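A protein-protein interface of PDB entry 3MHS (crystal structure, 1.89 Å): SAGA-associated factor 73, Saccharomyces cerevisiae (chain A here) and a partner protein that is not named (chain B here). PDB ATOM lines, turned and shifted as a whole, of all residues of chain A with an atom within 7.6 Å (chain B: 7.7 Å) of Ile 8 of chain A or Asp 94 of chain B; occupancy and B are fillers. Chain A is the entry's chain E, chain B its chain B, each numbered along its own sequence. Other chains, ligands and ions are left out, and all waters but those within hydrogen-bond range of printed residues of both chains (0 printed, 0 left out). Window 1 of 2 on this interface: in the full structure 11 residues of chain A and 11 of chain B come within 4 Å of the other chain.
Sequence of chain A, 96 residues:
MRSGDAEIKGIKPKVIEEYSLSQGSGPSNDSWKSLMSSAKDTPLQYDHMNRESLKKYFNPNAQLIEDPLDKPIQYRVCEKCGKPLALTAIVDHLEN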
ATOM      1  N   ASP A   5     -26.896 -13.158 -15.303  1.00  0.00           N
ATOM      2  CA  ASP A   5     -27.414 -13.606 -16.629  1.00  0.00           C
ATOM      3  C   ASP A   5     -28.546 -14.642 -16.500  1.00  0.00           C
ATOM      4  O   ASP A   5     -29.384 -14.759 -17.399  1.00  0.00           O
ATOM      5  CB  ASP A   5     -26.270 -14.168 -17.485  1.00  0.00           C
ATOM      6  CG  ASP A   5     -25.957 -15.629 -17.175  1.00  0.00           C
ATOM      7  OD1 ASP A   5     -25.695 -16.390 -18.133  1.00  0.00           O
ATOM      8  OD2 ASP A   5     -25.983 -16.019 -15.985  1.00  0.00           O
ATOM      9  N   ALA A   6     -28.561 -15.394 -15.395  1.00  0.00           N
ATOM     10  CA  ALA A   6     -29.602 -16.403 -15.148  1.00  0.00           C
ATOM     11  C   ALA A   6     -30.554 -15.950 -14.039  1.00  0.00           C
ATOM     12  O   ALA A   6     -30.353 -14.896 -13.426  1.00  0.00           O
ATOM     13  CB  ALA A   6     -28.974 -17.750 -14.793  1.00  0.00           C
ATOM     14  N   GLU A   7     -31.564 -16.774 -13.762  1.00  0.00           N
ATOM     15  CA  GLU A   7     -32.684 -16.382 -12.896  1.00  0.00           C
ATOM     16  C   GLU A   7     -32.463 -16.672 -11.401  1.00  0.00           C
ATOM     17  O   GLU A   7     -32.094 -17.781 -11.005  1.00  0.00           O
ATOM     18  CB  GLU A   7     -33.963 -17.060 -13.385  1.00  0.00           C
ATOM     19  CG  GLU A   7     -35.259 -16.398 -12.943  1.00  0.00           C
ATOM     20  CD  GLU A   7     -36.467 -16.945 -13.696  1.00  0.00           C
ATOM     21  OE1 GLU A   7     -37.613 -16.618 -13.323  1.00  0.00           O
ATOM     22  OE2 GLU A   7     -36.270 -17.702 -14.669  1.00  0.00           O
ATOM     23  N   ILE A   8     -32.725 -15.659 -10.578  1.00  0.00           N
ATOM     24  CA  ILE A   8     -32.494 -15.732  -9.137  1.00  0.00           C
ATOM     25  C   ILE A   8     -33.705 -16.320  -8.423  1.00  0.00           C
ATOM     26  O   ILE A   8     -34.843 -16.015  -8.767  1.00  0.00           O
ATOM     27  CB  ILE A   8     -32.156 -14.334  -8.560  1.00  0.00           C
ATOM     28  CG1 ILE A   8     -32.053 -14.371  -7.032  1.00  0.00           C
ATOM     29  CG2 ILE A   8     -33.193 -13.312  -8.994  1.00  0.00           C
ATOM     30  CD1 ILE A   8     -31.353 -13.152  -6.461  1.00  0.00           C
ATOM     31  N   LYS A   9     -33.451 -17.156  -7.423  1.00  0.00           N
ATOM     32  CA  LYS A   9     -34.522 -17.899  -6.762  1.00  0.00           C
ATOM     33  C   LYS A   9     -34.814 -17.408  -5.352  1.00  0.00           C
ATOM     34  O   LYS A   9     -35.975 -17.317  -4.951  1.00  0.00           O
ATOM     35  CB  LYS A   9     -34.202 -19.400  -6.746  1.00  0.00           C
ATOM     36  CG  LYS A   9     -34.596 -20.114  -8.036  1.00  0.00           C
ATOM     37  CD  LYS A   9     -36.113 -20.300  -8.137  1.00  0.00           C
ATOM     38  CE  LYS A   9     -36.674 -19.826  -9.486  1.00  0.00           C
ATOM     39  NZ  LYS A   9     -36.066 -20.505 -10.667  1.00  0.00           N
ATOM     40  N   GLY A  10     -33.771 -17.113  -4.590  1.00  0.00           N
ATOM     41  CA  GLY A  10     -33.958 -16.640  -3.226  1.00  0.00           C
ATOM     42  C   GLY A  10     -32.683 -16.095  -2.625  1.00  0.00           C
ATOM     43  O   GLY A  10     -31.681 -15.950  -3.319  1.00  0.00           O
ATOM     44  N   ILE A  11     -32.734 -15.785  -1.331  1.00  0.00           N
ATOM     45  CA  ILE A  11     -31.561 -15.345  -0.582  1.00  0.00           C
ATOM     46  C   ILE A  11     -31.042 -16.489   0.279  1.00  0.00           C
ATOM     47  O   ILE A  11     -31.763 -16.994   1.130  1.00  0.00           O
ATOM     48  CB  ILE A  11     -31.891 -14.141   0.347  1.00  0.00           C
ATOM     49  CG1 ILE A  11     -31.890 -12.832  -0.442  1.00  0.00           C
ATOM     50  CG2 ILE A  11     -30.878 -14.027   1.481  1.00  0.00           C
ATOM     51  CD1 ILE A  11     -32.229 -11.626   0.406  1.00  0.00           C
ATOM     52  N   LYS A  12     -29.784 -16.868   0.066  1.00  0.00           N
ATOM     53  CA  LYS A  12     -29.108 -17.886   0.879  1.00  0.00           C
ATOM     54  C   LYS A  12     -29.484 -17.825   2.367  1.00  0.00           C
ATOM     55  O   LYS A  12     -29.322 -16.786   3.001  1.00  0.00           O
ATOM     56  CB  LYS A  12     -27.587 -17.745   0.742  1.00  0.00           C
ATOM     57  CG  LYS A  12     -27.062 -18.098  -0.642  1.00  0.00           C
ATOM     58  CD  LYS A  12     -25.541 -18.151  -0.675  1.00  0.00           C
ATOM     59  CE  LYS A  12     -25.041 -18.392  -2.090  1.00  0.00           C
ATOM     60  NZ  LYS A  12     -23.575 -18.616  -2.142  1.00  0.00           N
ATOM     61  N   PRO A  13     -29.977 -18.951   2.923  1.00  0.00           N
ATOM     62  CA  PRO A  13     -30.357 -19.064   4.335  1.00  0.00           C
ATOM     63  C   PRO A  13     -29.307 -18.675   5.392  1.00  0.00           C
ATOM     64  O   PRO A  13     -29.692 -18.280   6.489  1.00  0.00           O
ATOM     65  CB  PRO A  13     -30.728 -20.543   4.470  1.00  0.00           C
ATOM     66  CG  PRO A  13     -31.287 -20.901   3.131  1.00  0.00           C
ATOM     67  CD  PRO A  13     -30.533 -20.065   2.124  1.00  0.00           C
ATOM     68  N   LYS A  14     -28.011 -18.792   5.100  1.00  0.00           N
ATOM     69  CA  LYS A  14     -26.989 -18.419   6.098  1.00  0.00           C
ATOM     70  C   LYS A  14     -26.856 -16.901   6.227  1.00  0.00           C
ATOM     71  O   LYS A  14     -26.468 -16.385   7.286  1.00  0.00           O
ATOM     72  CB  LYS A  14     -25.613 -19.014   5.774  1.00  0.00           C
ATOM     73  CG  LYS A  14     -24.550 -18.681   6.837  1.00  0.00           C
ATOM     74  CD  LYS A  14     -23.151 -19.126   6.433  1.00  0.00           C
ATOM     75  CE  LYS A  14     -22.347 -18.014   5.758  1.00  0.00           C
ATOM     76  NZ  LYS A  14     -21.850 -16.999   6.732  1.00  0.00           N
ATOM     77  N   LEU B   8     -37.672  -8.605  -1.984  1.00  0.00           N
ATOM     78  CA  LEU B   8     -36.346  -9.117  -2.272  1.00  0.00           C
ATOM     79  C   LEU B   8     -35.315  -8.000  -2.424  1.00  0.00           C
ATOM     80  O   LEU B   8     -34.241  -8.070  -1.828  1.00  0.00           O
ATOM     81  CB  LEU B   8     -36.369  -9.967  -3.535  1.00  0.00           C
ATOM     82  CG  LEU B   8     -35.121 -10.828  -3.715  1.00  0.00           C
ATOM     83  CD1 LEU B   8     -35.288 -12.172  -2.997  1.00  0.00           C
ATOM     84  CD2 LEU B   8     -34.833 -11.019  -5.193  1.00  0.00           C
ATOM     85  N   ILE B  12     -32.030  -7.706  -0.115  1.00  0.00           N
ATOM     86  CA  ILE B  12     -30.684  -7.729  -0.663  1.00  0.00           C
ATOM     87  C   ILE B  12     -29.889  -6.465  -0.294  1.00  0.00           C
ATOM     88  O   ILE B  12     -28.735  -6.558   0.099  1.00  0.00           O
ATOM     89  CB  ILE B  12     -30.727  -7.923  -2.202  1.00  0.00           C
ATOM     90  CG1 ILE B  12     -31.202  -9.353  -2.526  1.00  0.00           C
ATOM     91  CG2 ILE B  12     -29.361  -7.593  -2.838  1.00  0.00           C
ATOM     92  CD1 ILE B  12     -31.444  -9.632  -4.007  1.00  0.00           C
ATOM     93  N   LEU B  89     -23.481  -9.831  -5.166  1.00  0.00           N
ATOM     94  CA  LEU B  89     -24.801 -10.494  -5.206  1.00  0.00           C
ATOM     95  C   LEU B  89     -24.674 -12.013  -5.357  1.00  0.00           C
ATOM     96  O   LEU B  89     -25.376 -12.772  -4.695  1.00  0.00           O
ATOM     97  CB  LEU B  89     -25.647  -9.953  -6.362  1.00  0.00           C
ATOM     98  CG  LEU B  89     -26.280  -8.575  -6.193  1.00  0.00           C
ATOM     99  CD1 LEU B  89     -27.252  -8.334  -7.326  1.00  0.00           C
ATOM    100  CD2 LEU B  89     -26.980  -8.475  -4.850  1.00  0.00           C
ATOM    101  N   GLU B  90     -23.785 -12.446  -6.246  1.00  0.00           N
ATOM    102  CA  GLU B  90     -23.517 -13.878  -6.457  1.00  0.00           C
ATOM    103  C   GLU B  90     -22.984 -14.566  -5.201  1.00  0.00           C
ATOM    104  O   GLU B  90     -22.943 -15.787  -5.120  1.00  0.00           O
ATOM    105  CB  GLU B  90     -22.547 -14.068  -7.626  1.00  0.00           C
ATOM    106  CG  GLU B  90     -23.176 -13.688  -8.971  1.00  0.00           C
ATOM    107  CD  GLU B  90     -22.262 -13.933 -10.158  1.00  0.00           C
ATOM    108  OE1 GLU B  90     -21.076 -13.514 -10.103  1.00  0.00           O
ATOM    109  OE2 GLU B  90     -22.745 -14.527 -11.152  1.00  0.00           O
ATOM    110  N   GLU B  91     -22.608 -13.764  -4.216  1.00  0.00           N
ATOM    111  CA  GLU B  91     -22.181 -14.256  -2.914  1.00  0.00           C
ATOM    112  C   GLU B  91     -23.391 -14.810  -2.164  1.00  0.00           C
ATOM    113  O   GLU B  91     -23.353 -15.942  -1.689  1.00  0.00           O
ATOM    114  CB  GLU B  91     -21.551 -13.107  -2.114  1.00  0.00           C
ATOM    115  CG  GLU B  91     -20.268 -13.429  -1.351  1.00  0.00           C
ATOM    116  CD  GLU B  91     -19.267 -12.275  -1.399  1.00  0.00           C
ATOM    117  OE1 GLU B  91     -19.295 -11.389  -0.521  1.00  0.00           O
ATOM    118  OE2 GLU B  91     -18.463 -12.227  -2.346  1.00  0.00           O
ATOM    119  N   ILE B  92     -24.478 -14.034  -2.108  1.00  0.00           N
ATOM    120  CA  ILE B  92     -25.585 -14.337  -1.184  1.00  0.00           C
ATOM    121  C   ILE B  92     -26.981 -14.570  -1.768  1.00  0.00           C
ATOM    122  O   ILE B  92     -27.974 -14.523  -1.046  1.00  0.00           O
ATOM    123  CB  ILE B  92     -25.660 -13.281  -0.066  1.00  0.00           C
ATOM    124  CG1 ILE B  92     -25.930 -11.889  -0.648  1.00  0.00           C
ATOM    125  CG2 ILE B  92     -24.382 -13.326   0.741  1.00  0.00           C
ATOM    126  CD1 ILE B  92     -27.338 -11.378  -0.425  1.00  0.00           C
ATOM    127  N   VAL B  93     -27.058 -14.894  -3.053  1.00  0.00           N
ATOM    128  CA  VAL B  93     -28.300 -15.393  -3.614  1.00  0.00           C
ATOM    129  C   VAL B  93     -28.086 -16.741  -4.315  1.00  0.00           C
ATOM    130  O   VAL B  93     -27.055 -16.973  -4.953  1.00  0.00           O
ATOM    131  CB  VAL B  93     -28.931 -14.403  -4.606  1.00  0.00           C
ATOM    132  CG1 VAL B  93     -29.160 -13.044  -3.945  1.00  0.00           C
ATOM    133  CG2 VAL B  93     -28.086 -14.286  -5.867  1.00  0.00           C
ATOM    134  N   ASP B  94     -29.057 -17.636  -4.172  1.00  0.00           N
ATOM    135  CA  ASP B  94     -29.062 -18.863  -4.944  1.00  0.00           C
ATOM    136  C   ASP B  94     -29.781 -18.551  -6.244  1.00  0.00           C
ATOM    137  O   ASP B  94     -30.795 -17.857  -6.229  1.00  0.00           O
ATOM    138  CB  ASP B  94     -29.808 -19.963  -4.188  1.00  0.00           C
ATOM    139  CG  ASP B  94     -29.316 -20.131  -2.759  1.00  0.00           C
ATOM    140  OD1 ASP B  94     -28.096 -20.348  -2.577  1.00  0.00           O
ATOM    141  OD2 ASP B  94     -30.153 -20.066  -1.826  1.00  0.00           O
ATOM    142  N   THR B  95     -29.260 -19.032  -7.368  1.00  0.00           N
ATOM    143  CA  THR B  95     -29.981 -18.914  -8.641  1.00  0.00           C
ATOM    144  C   THR B  95     -30.261 -20.287  -9.260  1.00  0.00           C
ATOM    145  O   THR B  95     -30.283 -21.304  -8.566  1.00  0.00           O
ATOM    146  CB  THR B  95     -29.218 -18.029  -9.666  1.00  0.00           C
ATOM    147  OG1 THR B  95     -28.279 -18.824 -10.399  1.00  0.00           O
ATOM    148  CG2 THR B  95     -28.496 -16.856  -8.970  1.00  0.00           C
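Glu 7 of chain A touches Thr 95 of chain B (O to CB, 3.2 Å).
CB of Val 93 of chain B touches CD1 of Ile 8 of chain A (3.3 Å).
Asp 94 of chain B touches Ile 8 of chain A.
CB of Val 93 of chain B touches O of Gly 10 of chain A (3.4 Å).
CD1 of Ile 11 of chain A touches CG1 of Ile 12 of chain B, 3.8 Å away.
CA of Ile 11 of chain A touches O of Ile 92 of chain B, 3.7 Å away.
Lys 12 of chain A touches Val 93 of chain B (CE to O, 3.8 Å).
Lys 12 of chain A touches Asp 94 of chain B (CG to OD1, 3.1 Å).
Asp 94 of chain B touches Pro 13 of chain A.
The side-chain amino group of Lys 12 of chain A is in hydrogen-bond range of the backbone carbonyl oxygen of Glu 91 of chain B (2.7 Å).
The backbone carbonyl oxygen (O) of Ile 92 of chain B lies within hydrogen-bond range of the backbone NH (N) of Lys 12 of chain A, 3.2 Å away.
The backbone carbonyl oxygen of Asp 94 of chain B lies within hydrogen-bond range of the backbone NH of Lys 9 of chain A (3.0 Å).
N of Asp 94 of chain B lies within hydrogen-bond range of O of Gly 10 of chain A (3.2 Å).
Of the 9 printed residues of chain B, 6 touch a printed residue of chain A.
Hydrophobic or aromatic side chains of chain B that line the printed part of chain A: Ile 12 and Val 93.
Printed residues of chain A that touch a printed residue of chain B: Glu 7, Ile 8, Lys 9, Gly 10, Ile 11, Lys 12 and Pro 13.
Hydrophobic or aromatic side chains of chain A within 4 Å of the printed part of chain B: Ile 8, Ile 11 and Pro 13.
Among the printed residues, 13 pairs touch across the chains.
Among the printed residues, no Asp or Glu carboxylate lies within 4 Å of a Lys or Arg side-chain nitrogen of the other chain.
Of chain B, only Val 93 and Asp 94 come within 4 Å of Ile 8 of chain A.
Printed residues of chain A within 4 Å of Asp 94 of chain B: Ile 8 (3.8 Å), Lys 9 (3.0 Å), Gly 10 (3.2 Å), Lys 12 (3.1 Å) and Pro 13 (3.97 Å).
Of the printed residues of chain A, Thr 95 of chain B touches Glu 7 (3.2 Å).
Printed residues of chain B within 4 Å of Gly 10 of chain A: Val 93 and Asp 94.
Printed residues of chain A within 4 Å of Ile 92 of chain B: Ile 11 and Lys 12.
Of the printed residues of chain B, Lys 12 of chain A touches Glu 91, Ile 92, Val 93 and Asp 94.
Of the printed residues of chain A, Ile 12 of chain B touches Ile 11 (3.8 Å).
The nearest residue of chain A that does not touch Asp 94 of chain B is Ile 11 of chain A (4.2 Å).
The nearest printed residue of chain A that does not touch Ile 12 of chain B is Ile 8 of chain A (4.3 Å).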
